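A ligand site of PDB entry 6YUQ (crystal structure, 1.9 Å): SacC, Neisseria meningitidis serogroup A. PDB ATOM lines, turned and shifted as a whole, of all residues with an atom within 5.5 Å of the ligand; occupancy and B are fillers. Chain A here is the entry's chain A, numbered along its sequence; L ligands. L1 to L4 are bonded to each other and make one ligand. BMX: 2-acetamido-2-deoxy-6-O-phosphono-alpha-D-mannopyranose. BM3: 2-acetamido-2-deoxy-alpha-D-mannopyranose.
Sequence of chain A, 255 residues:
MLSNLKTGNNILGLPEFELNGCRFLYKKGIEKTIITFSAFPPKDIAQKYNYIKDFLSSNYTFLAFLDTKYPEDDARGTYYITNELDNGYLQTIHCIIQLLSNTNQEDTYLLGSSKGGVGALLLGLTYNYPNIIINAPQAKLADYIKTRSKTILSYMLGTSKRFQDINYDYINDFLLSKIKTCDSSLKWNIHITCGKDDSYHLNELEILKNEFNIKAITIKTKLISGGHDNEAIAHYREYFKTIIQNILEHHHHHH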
ATOM      1  N   SER A  38     -21.411 -29.236  -0.180  1.00  0.00           N
ATOM      2  CA  SER A  38     -21.408 -27.856   0.306  1.00  0.00           C
ATOM      3  C   SER A  38     -21.322 -26.879  -0.858  1.00  0.00           C
ATOM      4  O   SER A  38     -20.698 -27.148  -1.891  1.00  0.00           O
ATOM      5  CB  SER A  38     -20.228 -27.638   1.251  1.00  0.00           C
ATOM      6  OG  SER A  38     -20.042 -26.271   1.572  1.00  0.00           O
ATOM      7  N   ALA A  39     -21.957 -25.722  -0.679  1.00  0.00           N
ATOM      8  CA  ALA A  39     -21.889 -24.617  -1.631  1.00  0.00           C
ATOM      9  C   ALA A  39     -20.873 -23.570  -1.172  1.00  0.00           C
ATOM     10  O   ALA A  39     -20.272 -23.685  -0.099  1.00  0.00           O
ATOM     11  CB  ALA A  39     -23.262 -23.984  -1.816  1.00  0.00           C
ATOM     12  N   PHE A  40     -20.661 -22.550  -2.000  1.00  0.00           N
ATOM     13  CA  PHE A  40     -19.786 -21.421  -1.643  1.00  0.00           C
ATOM     14  C   PHE A  40     -20.409 -20.643  -0.496  1.00  0.00           C
ATOM     15  O   PHE A  40     -21.496 -20.076  -0.670  1.00  0.00           O
ATOM     16  CB  PHE A  40     -19.579 -20.453  -2.836  1.00  0.00           C
ATOM     17  CG  PHE A  40     -18.393 -20.796  -3.703  1.00  0.00           C
ATOM     18  CD1 PHE A  40     -17.214 -21.255  -3.145  1.00  0.00           C
ATOM     19  CD2 PHE A  40     -18.461 -20.636  -5.079  1.00  0.00           C
ATOM     20  CE1 PHE A  40     -16.117 -21.572  -3.942  1.00  0.00           C
ATOM     21  CE2 PHE A  40     -17.369 -20.953  -5.889  1.00  0.00           C
ATOM     22  CZ  PHE A  40     -16.195 -21.421  -5.314  1.00  0.00           C
ATOM     23  N   PRO A  41     -19.798 -20.589   0.679  1.00  0.00           N
ATOM     24  CA  PRO A  41     -20.304 -19.729   1.750  1.00  0.00           C
ATOM     25  C   PRO A  41     -19.881 -18.296   1.499  1.00  0.00           C
ATOM     26  O   PRO A  41     -19.035 -18.039   0.628  1.00  0.00           O
ATOM     27  CB  PRO A  41     -19.618 -20.304   2.992  1.00  0.00           C
ATOM     28  CG  PRO A  41     -18.293 -20.759   2.478  1.00  0.00           C
ATOM     29  CD  PRO A  41     -18.566 -21.295   1.077  1.00  0.00           C
ATOM     30  N   PRO A  42     -20.460 -17.320   2.215  1.00  0.00           N
ATOM     31  CA  PRO A  42     -19.976 -15.937   2.094  1.00  0.00           C
ATOM     32  C   PRO A  42     -18.523 -15.842   2.529  1.00  0.00           C
ATOM     33  O   PRO A  42     -17.999 -16.685   3.261  1.00  0.00           O
ATOM     34  CB  PRO A  42     -20.893 -15.141   3.040  1.00  0.00           C
ATOM     35  CG  PRO A  42     -22.110 -16.004   3.190  1.00  0.00           C
ATOM     36  CD  PRO A  42     -21.585 -17.419   3.160  1.00  0.00           C
ATOM     37  N   LYS A  43     -17.864 -14.772   2.086  1.00  0.00           N
ATOM     38  CA  LYS A  43     -16.450 -14.603   2.374  1.00  0.00           C
ATOM     39  C   LYS A  43     -16.228 -14.531   3.880  1.00  0.00           C
ATOM     40  O   LYS A  43     -17.036 -13.963   4.621  1.00  0.00           O
ATOM     41  CB  LYS A  43     -15.903 -13.336   1.700  1.00  0.00           C
ATOM     42  CG  LYS A  43     -14.442 -13.047   2.041  1.00  0.00           C
ATOM     43  CD  LYS A  43     -13.843 -11.961   1.159  1.00  0.00           C
ATOM     44  CE  LYS A  43     -12.581 -11.381   1.780  1.00  0.00           C
ATOM     45  NZ  LYS A  43     -11.455 -12.362   1.715  1.00  0.00           N
ATOM     46  N   LYS A  48     -19.907 -25.024   5.000  1.00  0.00           N
ATOM     47  CA  LYS A  48     -20.977 -25.580   5.815  1.00  0.00           C
ATOM     48  C   LYS A  48     -21.478 -26.903   5.231  1.00  0.00           C
ATOM     49  O   LYS A  48     -21.605 -27.039   4.009  1.00  0.00           O
ATOM     50  CB  LYS A  48     -22.136 -24.592   5.944  1.00  0.00           C
ATOM     51  N   TYR A  49     -21.747 -27.864   6.107  1.00  0.00           N
ATOM     52  CA  TYR A  49     -22.415 -29.082   5.693  1.00  0.00           C
ATOM     53  C   TYR A  49     -23.889 -28.802   5.447  1.00  0.00           C
ATOM     54  O   TYR A  49     -24.505 -28.004   6.153  1.00  0.00           O
ATOM     55  CB  TYR A  49     -22.245 -30.174   6.753  1.00  0.00           C
ATOM     56  CG  TYR A  49     -20.815 -30.599   6.946  1.00  0.00           C
ATOM     57  CD1 TYR A  49     -20.219 -31.506   6.085  1.00  0.00           C
ATOM     58  CD2 TYR A  49     -20.052 -30.097   8.002  1.00  0.00           C
ATOM     59  CE1 TYR A  49     -18.910 -31.905   6.246  1.00  0.00           C
ATOM     60  CE2 TYR A  49     -18.734 -30.508   8.183  1.00  0.00           C
ATOM     61  CZ  TYR A  49     -18.167 -31.406   7.295  1.00  0.00           C
ATOM     62  OH  TYR A  49     -16.866 -31.822   7.445  1.00  0.00           O
ATOM     63  N   ASN A  50     -24.453 -29.444   4.443  1.00  0.00           N
ATOM     64  CA  ASN A  50     -25.771 -29.093   3.941  1.00  0.00           C
ATOM     65  C   ASN A  50     -26.818 -30.133   4.337  1.00  0.00           C
ATOM     66  O   ASN A  50     -26.571 -31.345   4.265  1.00  0.00           O
ATOM     67  CB  ASN A  50     -25.741 -28.944   2.424  1.00  0.00           C
ATOM     68  CG  ASN A  50     -25.425 -27.535   1.979  1.00  0.00           C
ATOM     69  OD1 ASN A  50     -24.374 -26.976   2.310  1.00  0.00           O
ATOM     70  ND2 ASN A  50     -26.334 -26.942   1.241  1.00  0.00           N
ATOM     71  N   TYR A  51     -27.979 -29.633   4.758  1.00  0.00           N
ATOM     72  CA  TYR A  51     -29.211 -30.411   4.948  1.00  0.00           C
ATOM     73  C   TYR A  51     -29.094 -31.445   6.070  1.00  0.00           C
ATOM     74  O   TYR A  51     -29.777 -32.469   6.031  1.00  0.00           O
ATOM     75  CB  TYR A  51     -29.648 -31.076   3.643  1.00  0.00           C
ATOM     76  CG  TYR A  51     -29.520 -30.147   2.443  1.00  0.00           C
ATOM     77  CD1 TYR A  51     -29.956 -28.824   2.497  1.00  0.00           C
ATOM     78  CD2 TYR A  51     -28.953 -30.603   1.273  1.00  0.00           C
ATOM     79  CE1 TYR A  51     -29.819 -27.973   1.409  1.00  0.00           C
ATOM     80  CE2 TYR A  51     -28.805 -29.780   0.175  1.00  0.00           C
ATOM     81  CZ  TYR A  51     -29.239 -28.473   0.244  1.00  0.00           C
ATOM     82  OH  TYR A  51     -29.069 -27.679  -0.875  1.00  0.00           O
ATOM     83  N   LYS A  53     -30.228 -31.064   9.155  1.00  0.00           N
ATOM     84  CA  LYS A  53     -31.467 -31.130   9.922  1.00  0.00           C
ATOM     85  C   LYS A  53     -32.583 -31.847   9.177  1.00  0.00           C
ATOM     86  O   LYS A  53     -33.527 -32.329   9.822  1.00  0.00           O
ATOM     87  CB  LYS A  53     -31.909 -29.720  10.321  1.00  0.00           C
ATOM     88  CG  LYS A  53     -30.794 -28.841  10.871  1.00  0.00           C
ATOM     89  CD  LYS A  53     -31.355 -27.524  11.386  1.00  0.00           C
ATOM     90  CE  LYS A  53     -30.250 -26.510  11.655  1.00  0.00           C
ATOM     91  NZ  LYS A  53     -30.768 -25.111  11.713  1.00  0.00           N
ATOM     92  N   ARG A  76     -12.653 -21.466   0.631  1.00  0.00           N
ATOM     93  CA  ARG A  76     -14.032 -21.869   0.370  1.00  0.00           C
ATOM     94  C   ARG A  76     -14.153 -22.931  -0.703  1.00  0.00           C
ATOM     95  O   ARG A  76     -15.275 -23.265  -1.099  1.00  0.00           O
ATOM     96  CB  ARG A  76     -14.863 -20.635   0.000  1.00  0.00           C
ATOM     97  CG  ARG A  76     -15.060 -19.716   1.188  1.00  0.00           C
ATOM     98  CD  ARG A  76     -15.870 -18.479   0.825  1.00  0.00           C
ATOM     99  NE  ARG A  76     -15.087 -17.479   0.090  1.00  0.00           N
ATOM    100  CZ  ARG A  76     -15.643 -16.495  -0.612  1.00  0.00           C
ATOM    101  NH1 ARG A  76     -16.954 -16.369  -0.671  1.00  0.00           N
ATOM    102  NH2 ARG A  76     -14.866 -15.611  -1.235  1.00  0.00           N
ATOM    103  N   SER A 113     -26.999 -27.560  -3.774  1.00  0.00           N
ATOM    104  CA  SER A 113     -27.493 -26.368  -4.455  1.00  0.00           C
ATOM    105  C   SER A 113     -26.312 -25.512  -4.885  1.00  0.00           C
ATOM    106  O   SER A 113     -25.297 -25.441  -4.168  1.00  0.00           O
ATOM    107  CB  SER A 113     -28.455 -25.573  -3.546  1.00  0.00           C
ATOM    108  OG  SER A 113     -28.862 -24.362  -4.169  1.00  0.00           O
ATOM    109  N   SER A 114     -26.425 -24.881  -6.053  1.00  0.00           N
ATOM    110  CA  SER A 114     -25.377 -23.988  -6.595  1.00  0.00           C
ATOM    111  C   SER A 114     -24.092 -24.791  -6.755  1.00  0.00           C
ATOM    112  O   SER A 114     -24.112 -25.793  -7.491  1.00  0.00           O
ATOM    113  CB  SER A 114     -25.272 -22.754  -5.703  1.00  0.00           C
ATOM    114  OG  SER A 114     -24.581 -21.703  -6.369  1.00  0.00           O
ATOM    115  N   LYS A 115     -22.977 -24.390  -6.140  1.00  0.00           N
ATOM    116  CA  LYS A 115     -21.738 -25.163  -6.263  1.00  0.00           C
ATOM    117  C   LYS A 115     -21.939 -26.586  -5.747  1.00  0.00           C
ATOM    118  O   LYS A 115     -21.341 -27.532  -6.267  1.00  0.00           O
ATOM    119  CB  LYS A 115     -20.601 -24.484  -5.509  1.00  0.00           C
ATOM    120  CG  LYS A 115     -19.247 -25.205  -5.653  1.00  0.00           C
ATOM    121  CD  LYS A 115     -18.179 -24.619  -4.735  1.00  0.00           C
ATOM    122  CE  LYS A 115     -18.359 -25.078  -3.293  1.00  0.00           C
ATOM    123  NZ  LYS A 115     -17.203 -24.711  -2.428  1.00  0.00           N
ATOM    124  N   ASN A 135     -30.319 -28.101  -7.010  1.00  0.00           N
ATOM    125  CA  ASN A 135     -30.924 -26.805  -7.285  1.00  0.00           C
ATOM    126  C   ASN A 135     -29.885 -25.864  -7.886  1.00  0.00           C
ATOM    127  O   ASN A 135     -28.732 -25.852  -7.451  1.00  0.00           O
ATOM    128  CB  ASN A 135     -31.515 -26.180  -6.023  1.00  0.00           C
ATOM    129  CG  ASN A 135     -32.093 -24.799  -6.281  1.00  0.00           C
ATOM    130  OD1 ASN A 135     -33.131 -24.667  -6.923  1.00  0.00           O
ATOM    131  ND2 ASN A 135     -31.407 -23.773  -5.799  1.00  0.00           N
ATOM    132  N   TYR A 144     -18.646 -18.178 -13.123  1.00  0.00           N
ATOM    133  CA  TYR A 144     -19.307 -17.982 -11.848  1.00  0.00           C
ATOM    134  C   TYR A 144     -18.318 -17.736 -10.721  1.00  0.00           C
ATOM    135  O   TYR A 144     -18.571 -16.901  -9.848  1.00  0.00           O
ATOM    136  CB  TYR A 144     -20.201 -19.171 -11.510  1.00  0.00           C
ATOM    137  CG  TYR A 144     -20.967 -18.963 -10.211  1.00  0.00           C
ATOM    138  CD1 TYR A 144     -22.059 -18.098 -10.162  1.00  0.00           C
ATOM    139  CD2 TYR A 144     -20.603 -19.620  -9.045  1.00  0.00           C
ATOM    140  CE1 TYR A 144     -22.772 -17.891  -8.989  1.00  0.00           C
ATOM    141  CE2 TYR A 144     -21.305 -19.419  -7.860  1.00  0.00           C
ATOM    142  CZ  TYR A 144     -22.393 -18.557  -7.835  1.00  0.00           C
ATOM    143  OH  TYR A 144     -23.097 -18.353  -6.672  1.00  0.00           O
ATOM    144  N   LYS A 146     -15.580 -16.272 -10.979  1.00  0.00           N
ATOM    145  CA  LYS A 146     -15.164 -14.889 -11.166  1.00  0.00           C
ATOM    146  C   LYS A 146     -16.067 -13.934 -10.413  1.00  0.00           C
ATOM    147  O   LYS A 146     -15.604 -12.932  -9.854  1.00  0.00           O
ATOM    148  CB  LYS A 146     -15.156 -14.550 -12.660  1.00  0.00           C
ATOM    149  CG  LYS A 146     -14.401 -13.300 -13.018  1.00  0.00           C
ATOM    150  CD  LYS A 146     -14.155 -13.227 -14.513  1.00  0.00           C
ATOM    151  CE  LYS A 146     -15.422 -12.897 -15.267  1.00  0.00           C
ATOM    152  NZ  LYS A 146     -15.118 -11.984 -16.403  1.00  0.00           N
ATOM    153  N   THR A 147     -17.361 -14.226 -10.370  1.00  0.00           N
ATOM    154  CA  THR A 147     -18.324 -13.356  -9.690  1.00  0.00           C
ATOM    155  C   THR A 147     -18.394 -13.588  -8.193  1.00  0.00           C
ATOM    156  O   THR A 147     -19.155 -12.894  -7.512  1.00  0.00           O
ATOM    157  CB  THR A 147     -19.728 -13.543 -10.275  1.00  0.00           C
ATOM    158  OG1 THR A 147     -20.320 -14.712  -9.702  1.00  0.00           O
ATOM    159  CG2 THR A 147     -19.671 -13.695 -11.790  1.00  0.00           C
ATOM    160  N   ARG A 148     -17.635 -14.540  -7.649  1.00  0.00           N
ATOM    161  CA  ARG A 148     -17.702 -14.882  -6.231  1.00  0.00           C
ATOM    162  C   ARG A 148     -16.406 -14.632  -5.481  1.00  0.00           C
ATOM    163  O   ARG A 148     -16.441 -14.199  -4.325  1.00  0.00           O
ATOM    164  CB  ARG A 148     -18.103 -16.358  -6.054  1.00  0.00           C
ATOM    165  CG  ARG A 148     -19.568 -16.641  -6.334  1.00  0.00           C
ATOM    166  CD  ARG A 148     -20.488 -15.754  -5.482  1.00  0.00           C
ATOM    167  NE  ARG A 148     -20.300 -16.003  -4.048  1.00  0.00           N
ATOM    168  CZ  ARG A 148     -20.843 -17.038  -3.415  1.00  0.00           C
ATOM    169  NH1 ARG A 148     -21.590 -17.902  -4.086  1.00  0.00           N
ATOM    170  NH2 ARG A 148     -20.623 -17.207  -2.117  1.00  0.00           N
ATOM    171  N   SER A 149     -15.240 -14.901  -6.094  1.00  0.00           N
ATOM    172  CA  SER A 149     -13.961 -14.669  -5.427  1.00  0.00           C
ATOM    173  C   SER A 149     -12.871 -14.648  -6.492  1.00  0.00           C
ATOM    174  O   SER A 149     -12.597 -15.683  -7.116  1.00  0.00           O
ATOM    175  CB  SER A 149     -13.676 -15.750  -4.388  1.00  0.00           C
ATOM    176  OG  SER A 149     -12.289 -15.872  -4.153  1.00  0.00           O
ATOM    177  N   LYS A 150     -12.240 -13.489  -6.665  1.00  0.00           N
ATOM    178  CA  LYS A 150     -11.087 -13.420  -7.559  1.00  0.00           C
ATOM    179  C   LYS A 150      -9.913 -14.217  -7.015  1.00  0.00           C
ATOM    180  O   LYS A 150      -9.107 -14.752  -7.787  1.00  0.00           O
ATOM    181  CB  LYS A 150     -10.692 -11.961  -7.793  1.00  0.00           C
ATOM    182  CG  LYS A 150     -11.762 -11.145  -8.518  1.00  0.00           C
ATOM    183  CD  LYS A 150     -11.867 -11.516  -9.995  1.00  0.00           C
ATOM    184  CE  LYS A 150     -12.702 -10.518 -10.792  1.00  0.00           C
ATOM    185  NZ  LYS A 150     -14.142 -10.530 -10.413  1.00  0.00           N
ATOM    186  N   GLY A 227     -35.247 -16.559  -5.849  1.00  0.00           N
ATOM    187  CA  GLY A 227     -34.082 -16.374  -6.691  1.00  0.00           C
ATOM    188  C   GLY A 227     -32.995 -17.357  -6.327  1.00  0.00           C
ATOM    189  O   GLY A 227     -33.294 -18.537  -6.071  1.00  0.00           O
ATOM    190  N   HIS A 228     -31.740 -16.898  -6.316  1.00  0.00           N
ATOM    191  CA  HIS A 228     -30.607 -17.667  -5.804  1.00  0.00           C
ATOM    192  C   HIS A 228     -30.408 -17.338  -4.323  1.00  0.00           C
ATOM    193  O   HIS A 228     -29.412 -16.754  -3.913  1.00  0.00           O
ATOM    194  CB  HIS A 228     -29.347 -17.355  -6.611  1.00  0.00           C
ATOM    195  CG  HIS A 228     -28.333 -18.452  -6.653  1.00  0.00           C
ATOM    196  ND1 HIS A 228     -28.415 -19.507  -7.537  1.00  0.00           N
ATOM    197  CD2 HIS A 228     -27.208 -18.656  -5.919  1.00  0.00           C
ATOM    198  CE1 HIS A 228     -27.381 -20.315  -7.341  1.00  0.00           C
ATOM    199  NE2 HIS A 228     -26.639 -19.820  -6.375  1.00  0.00           N
ATOM    200  N   ASP A 229     -31.381 -17.767  -3.518  1.00  0.00           N
ATOM    201  CA  ASP A 229     -31.476 -17.302  -2.130  1.00  0.00           C
ATOM    202  C   ASP A 229     -32.057 -18.422  -1.261  1.00  0.00           C
ATOM    203  O   ASP A 229     -32.255 -19.547  -1.716  1.00  0.00           O
ATOM    204  CB  ASP A 229     -32.350 -16.038  -2.056  1.00  0.00           C
ATOM    205  CG  ASP A 229     -33.687 -16.228  -2.764  1.00  0.00           C
ATOM    206  OD1 ASP A 229     -34.254 -17.333  -2.684  1.00  0.00           O
ATOM    207  OD2 ASP A 229     -34.163 -15.272  -3.411  1.00  0.00           O
ATOM    208  N   ASN A 230     -32.367 -18.078  -0.008  1.00  0.00           N
ATOM    209  CA  ASN A 230     -32.886 -19.046   0.946  1.00  0.00           C
ATOM    210  C   ASN A 230     -34.323 -19.477   0.654  1.00  0.00           C
ATOM    211  O   ASN A 230     -34.725 -20.564   1.080  1.00  0.00           O
ATOM    212  CB  ASN A 230     -32.798 -18.459   2.367  1.00  0.00           C
ATOM    213  CG  ASN A 230     -31.415 -18.650   2.983  1.00  0.00           C
ATOM    214  OD1 ASN A 230     -30.437 -18.950   2.289  1.00  0.00           O
ATOM    215  ND2 ASN A 230     -31.340 -18.492   4.306  1.00  0.00           N
ATOM    216  N   ILE A 233     -33.997 -22.323  -1.755  1.00  0.00           N
ATOM    217  CA  ILE A 233     -33.471 -23.466  -1.005  1.00  0.00           C
ATOM    218  C   ILE A 233     -34.573 -24.117  -0.189  1.00  0.00           C
ATOM    219  O   ILE A 233     -34.665 -25.351  -0.113  1.00  0.00           O
ATOM    220  CB  ILE A 233     -32.283 -23.033  -0.132  1.00  0.00           C
ATOM    221  CG1 ILE A 233     -31.013 -22.875  -0.982  1.00  0.00           C
ATOM    222  CG2 ILE A 233     -32.021 -24.056   0.967  1.00  0.00           C
ATOM    223  CD1 ILE A 233     -29.919 -22.124  -0.283  1.00  0.00           C
ATOM    224  N   ARG A 237     -35.622 -27.934  -0.645  1.00  0.00           N
ATOM    225  CA  ARG A 237     -35.686 -28.912   0.444  1.00  0.00           C
ATOM    226  C   ARG A 237     -37.014 -29.664   0.434  1.00  0.00           C
ATOM    227  O   ARG A 237     -37.055 -30.880   0.604  1.00  0.00           O
ATOM    228  CB  ARG A 237     -35.484 -28.207   1.796  1.00  0.00           C
ATOM    229  CG  ARG A 237     -34.025 -27.918   2.183  1.00  0.00           C
ATOM    230  CD  ARG A 237     -33.911 -27.191   3.521  1.00  0.00           C
ATOM    231  NE  ARG A 237     -33.626 -28.072   4.666  1.00  0.00           N
ATOM    232  CZ  ARG A 237     -32.773 -27.768   5.645  1.00  0.00           C
ATOM    233  NH1 ARG A 237     -32.569 -28.608   6.636  1.00  0.00           N
ATOM    234  NH2 ARG A 237     -32.098 -26.633   5.600  1.00  0.00           N
HETATM  235  C1  BMX L   1     -27.721 -23.599   5.957  1.00  0.00           C
HETATM  236  C2  BMX L   1     -29.100 -22.972   6.069  1.00  0.00           C
HETATM  237  C3  BMX L   1     -29.368 -21.971   4.981  1.00  0.00           C
HETATM  238  C4  BMX L   1     -28.298 -21.940   3.916  1.00  0.00           C
HETATM  239  C5  BMX L   1     -27.855 -23.342   3.486  1.00  0.00           C
HETATM  240  C6  BMX L   1     -26.608 -23.253   2.617  1.00  0.00           C
HETATM  241  C7  BMX L   1     -30.181 -22.880   8.415  1.00  0.00           C
HETATM  242  C8  BMX L   1     -31.040 -24.131   8.057  1.00  0.00           C
HETATM  243  N2  BMX L   1     -29.231 -22.326   7.425  1.00  0.00           N
HETATM  244  O1  BMX L   1     -27.541 -24.509   6.976  1.00  0.00           O
HETATM  245  O3  BMX L   1     -29.509 -20.646   5.560  1.00  0.00           O
HETATM  246  O4  BMX L   1     -28.785 -21.209   2.776  1.00  0.00           O
HETATM  247  O5  BMX L   1     -27.565 -24.255   4.615  1.00  0.00           O
HETATM  248  O6  BMX L   1     -26.015 -21.948   2.777  1.00  0.00           O
HETATM  249  O7  BMX L   1     -30.282 -22.385   9.480  1.00  0.00           O
HETATM  250  P   BMX L   1     -24.464 -21.662   2.142  1.00  0.00           P
HETATM  251  O19 BMX L   1     -23.572 -22.847   2.428  1.00  0.00           O
HETATM  252  O17 BMX L   1     -23.862 -20.433   2.799  1.00  0.00           O
HETATM  253  O18 BMX L   1     -24.581 -21.444   0.503  1.00  0.00           O
HETATM  254  C1  BMX L   2     -25.695 -20.870  -0.023  1.00  0.00           C
HETATM  255  C2  BMX L   2     -25.580 -20.904  -1.541  1.00  0.00           C
HETATM  256  C3  BMX L   2     -24.504 -20.024  -2.047  1.00  0.00           C
HETATM  257  C4  BMX L   2     -24.641 -18.621  -1.496  1.00  0.00           C
HETATM  258  C5  BMX L   2     -24.664 -18.662   0.044  1.00  0.00           C
HETATM  259  C6  BMX L   2     -24.753 -17.282   0.632  1.00  0.00           C
HETATM  260  C7  BMX L   2     -27.700 -21.329  -2.917  1.00  0.00           C
HETATM  261  C8  BMX L   2     -28.992 -20.810  -3.556  1.00  0.00           C
HETATM  262  N2  BMX L   2     -26.850 -20.411  -2.165  1.00  0.00           N
HETATM  263  O3  BMX L   2     -24.562 -20.010  -3.497  1.00  0.00           O
HETATM  264  O4  BMX L   2     -23.569 -17.816  -1.938  1.00  0.00           O
HETATM  265  O5  BMX L   2     -25.807 -19.468   0.512  1.00  0.00           O
HETATM  266  O6  BMX L   2     -25.794 -16.558  -0.063  1.00  0.00           O
HETATM  267  O7  BMX L   2     -27.384 -22.482  -3.031  1.00  0.00           O
HETATM  268  P   BMX L   2     -26.723 -15.483   0.815  1.00  0.00           P
HETATM  269  O19 BMX L   2     -26.659 -15.850   2.291  1.00  0.00           O
HETATM  270  O17 BMX L   2     -28.158 -15.505   0.318  1.00  0.00           O
HETATM  271  O18 BMX L   2     -26.078 -13.939   0.614  1.00  0.00           O
HETATM  272  C1  BMX L   3     -24.942 -13.631   1.338  1.00  0.00           C
HETATM  273  C2  BMX L   3     -24.821 -12.131   1.466  1.00  0.00           C
HETATM  274  C3  BMX L   3     -24.706 -11.491   0.147  1.00  0.00           C
HETATM  275  C4  BMX L   3     -23.580 -12.076  -0.665  1.00  0.00           C
HETATM  276  C5  BMX L   3     -23.617 -13.603  -0.726  1.00  0.00           C
HETATM  277  C6  BMX L   3     -22.308 -14.088  -1.330  1.00  0.00           C
HETATM  278  C7  BMX L   3     -23.654 -11.350   3.652  1.00  0.00           C
HETATM  279  C8  BMX L   3     -25.023 -11.108   4.310  1.00  0.00           C
HETATM  280  N2  BMX L   3     -23.565 -11.837   2.274  1.00  0.00           N
HETATM  281  O3  BMX L   3     -24.494 -10.058   0.312  1.00  0.00           O
HETATM  282  O4  BMX L   3     -23.656 -11.543  -2.001  1.00  0.00           O
HETATM  283  O5  BMX L   3     -23.773 -14.215   0.608  1.00  0.00           O
HETATM  284  O6  BMX L   3     -21.270 -13.616  -0.479  1.00  0.00           O
HETATM  285  O7  BMX L   3     -22.651 -11.136   4.255  1.00  0.00           O
HETATM  286  P   BMX L   3     -19.720 -13.494  -1.106  1.00  0.00           P
HETATM  287  O19 BMX L   3     -19.080 -14.854  -1.075  1.00  0.00           O
HETATM  288  O17 BMX L   3     -18.818 -12.562  -0.344  1.00  0.00           O
HETATM  289  O18 BMX L   3     -19.862 -13.124  -2.742  1.00  0.00           O
HETATM  290  C1  BM3 L   4     -19.816 -11.843  -3.225  1.00  0.00           C
HETATM  291  C2  BM3 L   4     -20.615 -11.809  -4.524  1.00  0.00           C
HETATM  292  N2  BM3 L   4     -22.055 -12.252  -4.347  1.00  0.00           N
HETATM  293  C7  BM3 L   4     -22.787 -12.807  -5.503  1.00  0.00           C
HETATM  294  O7  BM3 L   4     -22.248 -12.884  -6.565  1.00  0.00           O
HETATM  295  C8  BM3 L   4     -24.276 -13.288  -5.336  1.00  0.00           C
HETATM  296  C3  BM3 L   4     -20.540 -10.446  -5.119  1.00  0.00           C
HETATM  297  O3  BM3 L   4     -21.151  -9.484  -4.210  1.00  0.00           O
HETATM  298  C4  BM3 L   4     -19.112 -10.042  -5.344  1.00  0.00           C
HETATM  299  O4  BM3 L   4     -18.965  -9.821  -6.756  1.00  0.00           O
HETATM  300  C5  BM3 L   4     -18.123 -11.129  -4.864  1.00  0.00           C
HETATM  301  C6  BM3 L   4     -16.667 -10.673  -4.995  1.00  0.00           C
HETATM  302  O6  BM3 L   4     -16.170 -11.203  -6.211  1.00  0.00           O
HETATM  303  O5  BM3 L   4     -18.368 -11.510  -3.469  1.00  0.00           O
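The guanidinium group of Arg 76 is in salt-bridge range of an oxygen (O19) of BMX L3. An oxygen (O7) of BMX L2 is in hydrogen-bond range of the side-chain hydroxyl of Ser 113 (2.6 Å). An oxygen (O4) of BMX L1 lies within hydrogen-bond range of the side-chain amide oxygen (OD1) of Asn 230. The guanidinium group (NH2) of Arg 148 is in salt-bridge range of an oxygen (O19) of BMX L3, at 3.0 Å. An oxygen (O4) of BM3 L4 is in hydrogen-bond range of the backbone carbonyl oxygen (O) of Thr 147, at 3.2 Å. An oxygen (O4) of BMX L2 sits close to the backbone carbonyl oxygen (O) of Phe 40 (3.3 Å). An oxygen (O3) of BMX L2 sits at hydrogen-bond distance from the side-chain hydroxyl (OG) of Ser 114 (3.3 Å). The backbone NH of Lys 43 lies within hydrogen-bond range of an oxygen (O19) of BMX L3, at 3.4 Å.
O of Arg 76 is in hydrogen-bond range of NZ of Lys 115 (2.8 Å). The side-chain hydroxyl (OG) of Ser 113 is in hydrogen-bond range of the side-chain amide nitrogen (ND2) of Asn 135. The guanidinium group of Arg 148 is in hydrogen-bond range of the backbone carbonyl oxygen of Phe 40 (3.3 Å). NH2 of Arg 148 sits at hydrogen-bond distance from O of Pro 41 (3.3 Å). The side-chain hydroxyl (OH) of Tyr 144 lies within hydrogen-bond range of the guanidinium group (NH1) of Arg 148 (3.0 Å). The backbone NH (N) of Ser 114 lies within hydrogen-bond range of the backbone carbonyl oxygen (O) of Asn 135 (2.9 Å). OD2 of Asp 229 lies within hydrogen-bond range of N of Gly 227, at 3.0 Å. The backbone carbonyl oxygen of Lys 48 sits close to the side-chain amide oxygen of Asn 50, 3.2 Å away.
CB of Ala 39 touches O18 of BMX L1, at 3.7 Å. O of Pro 41 touches O19 of BMX L3, 3.6 Å away. Pro 42 touches the ligand. ND2 of Asn 50 touches C6 of BMX L1, 3.9 Å away. Lys 53 touches the ligand. OH of Tyr 144 touches O3 of BMX L2, at 3.9 Å. Ser 149 touches the ligand. NE2 of His 228 touches O3 of BMX L2, at 3.6 Å. N of Asp 229 touches C8 of BMX L2 (3.9 Å). CD1 of Ile 233 touches O4 of BMX L1, 3.4 Å away. Arg 237 touches the ligand. Hydrophobic or aromatic side chains within 4 Å of the ligand: Ala 39, Pro 42, His 228 and Ile 233. 19 residues have an atom within 4 Å of the ligand: Ala 39, Phe 40, Pro 41, Pro 42, Lys 43, Asn 50, Lys 53, Arg 76, Ser 113, Ser 114, Tyr 144, Thr 147, Arg 148, Ser 149, His 228, Asp 229, Asn 230, Ile 233 and Arg 237.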
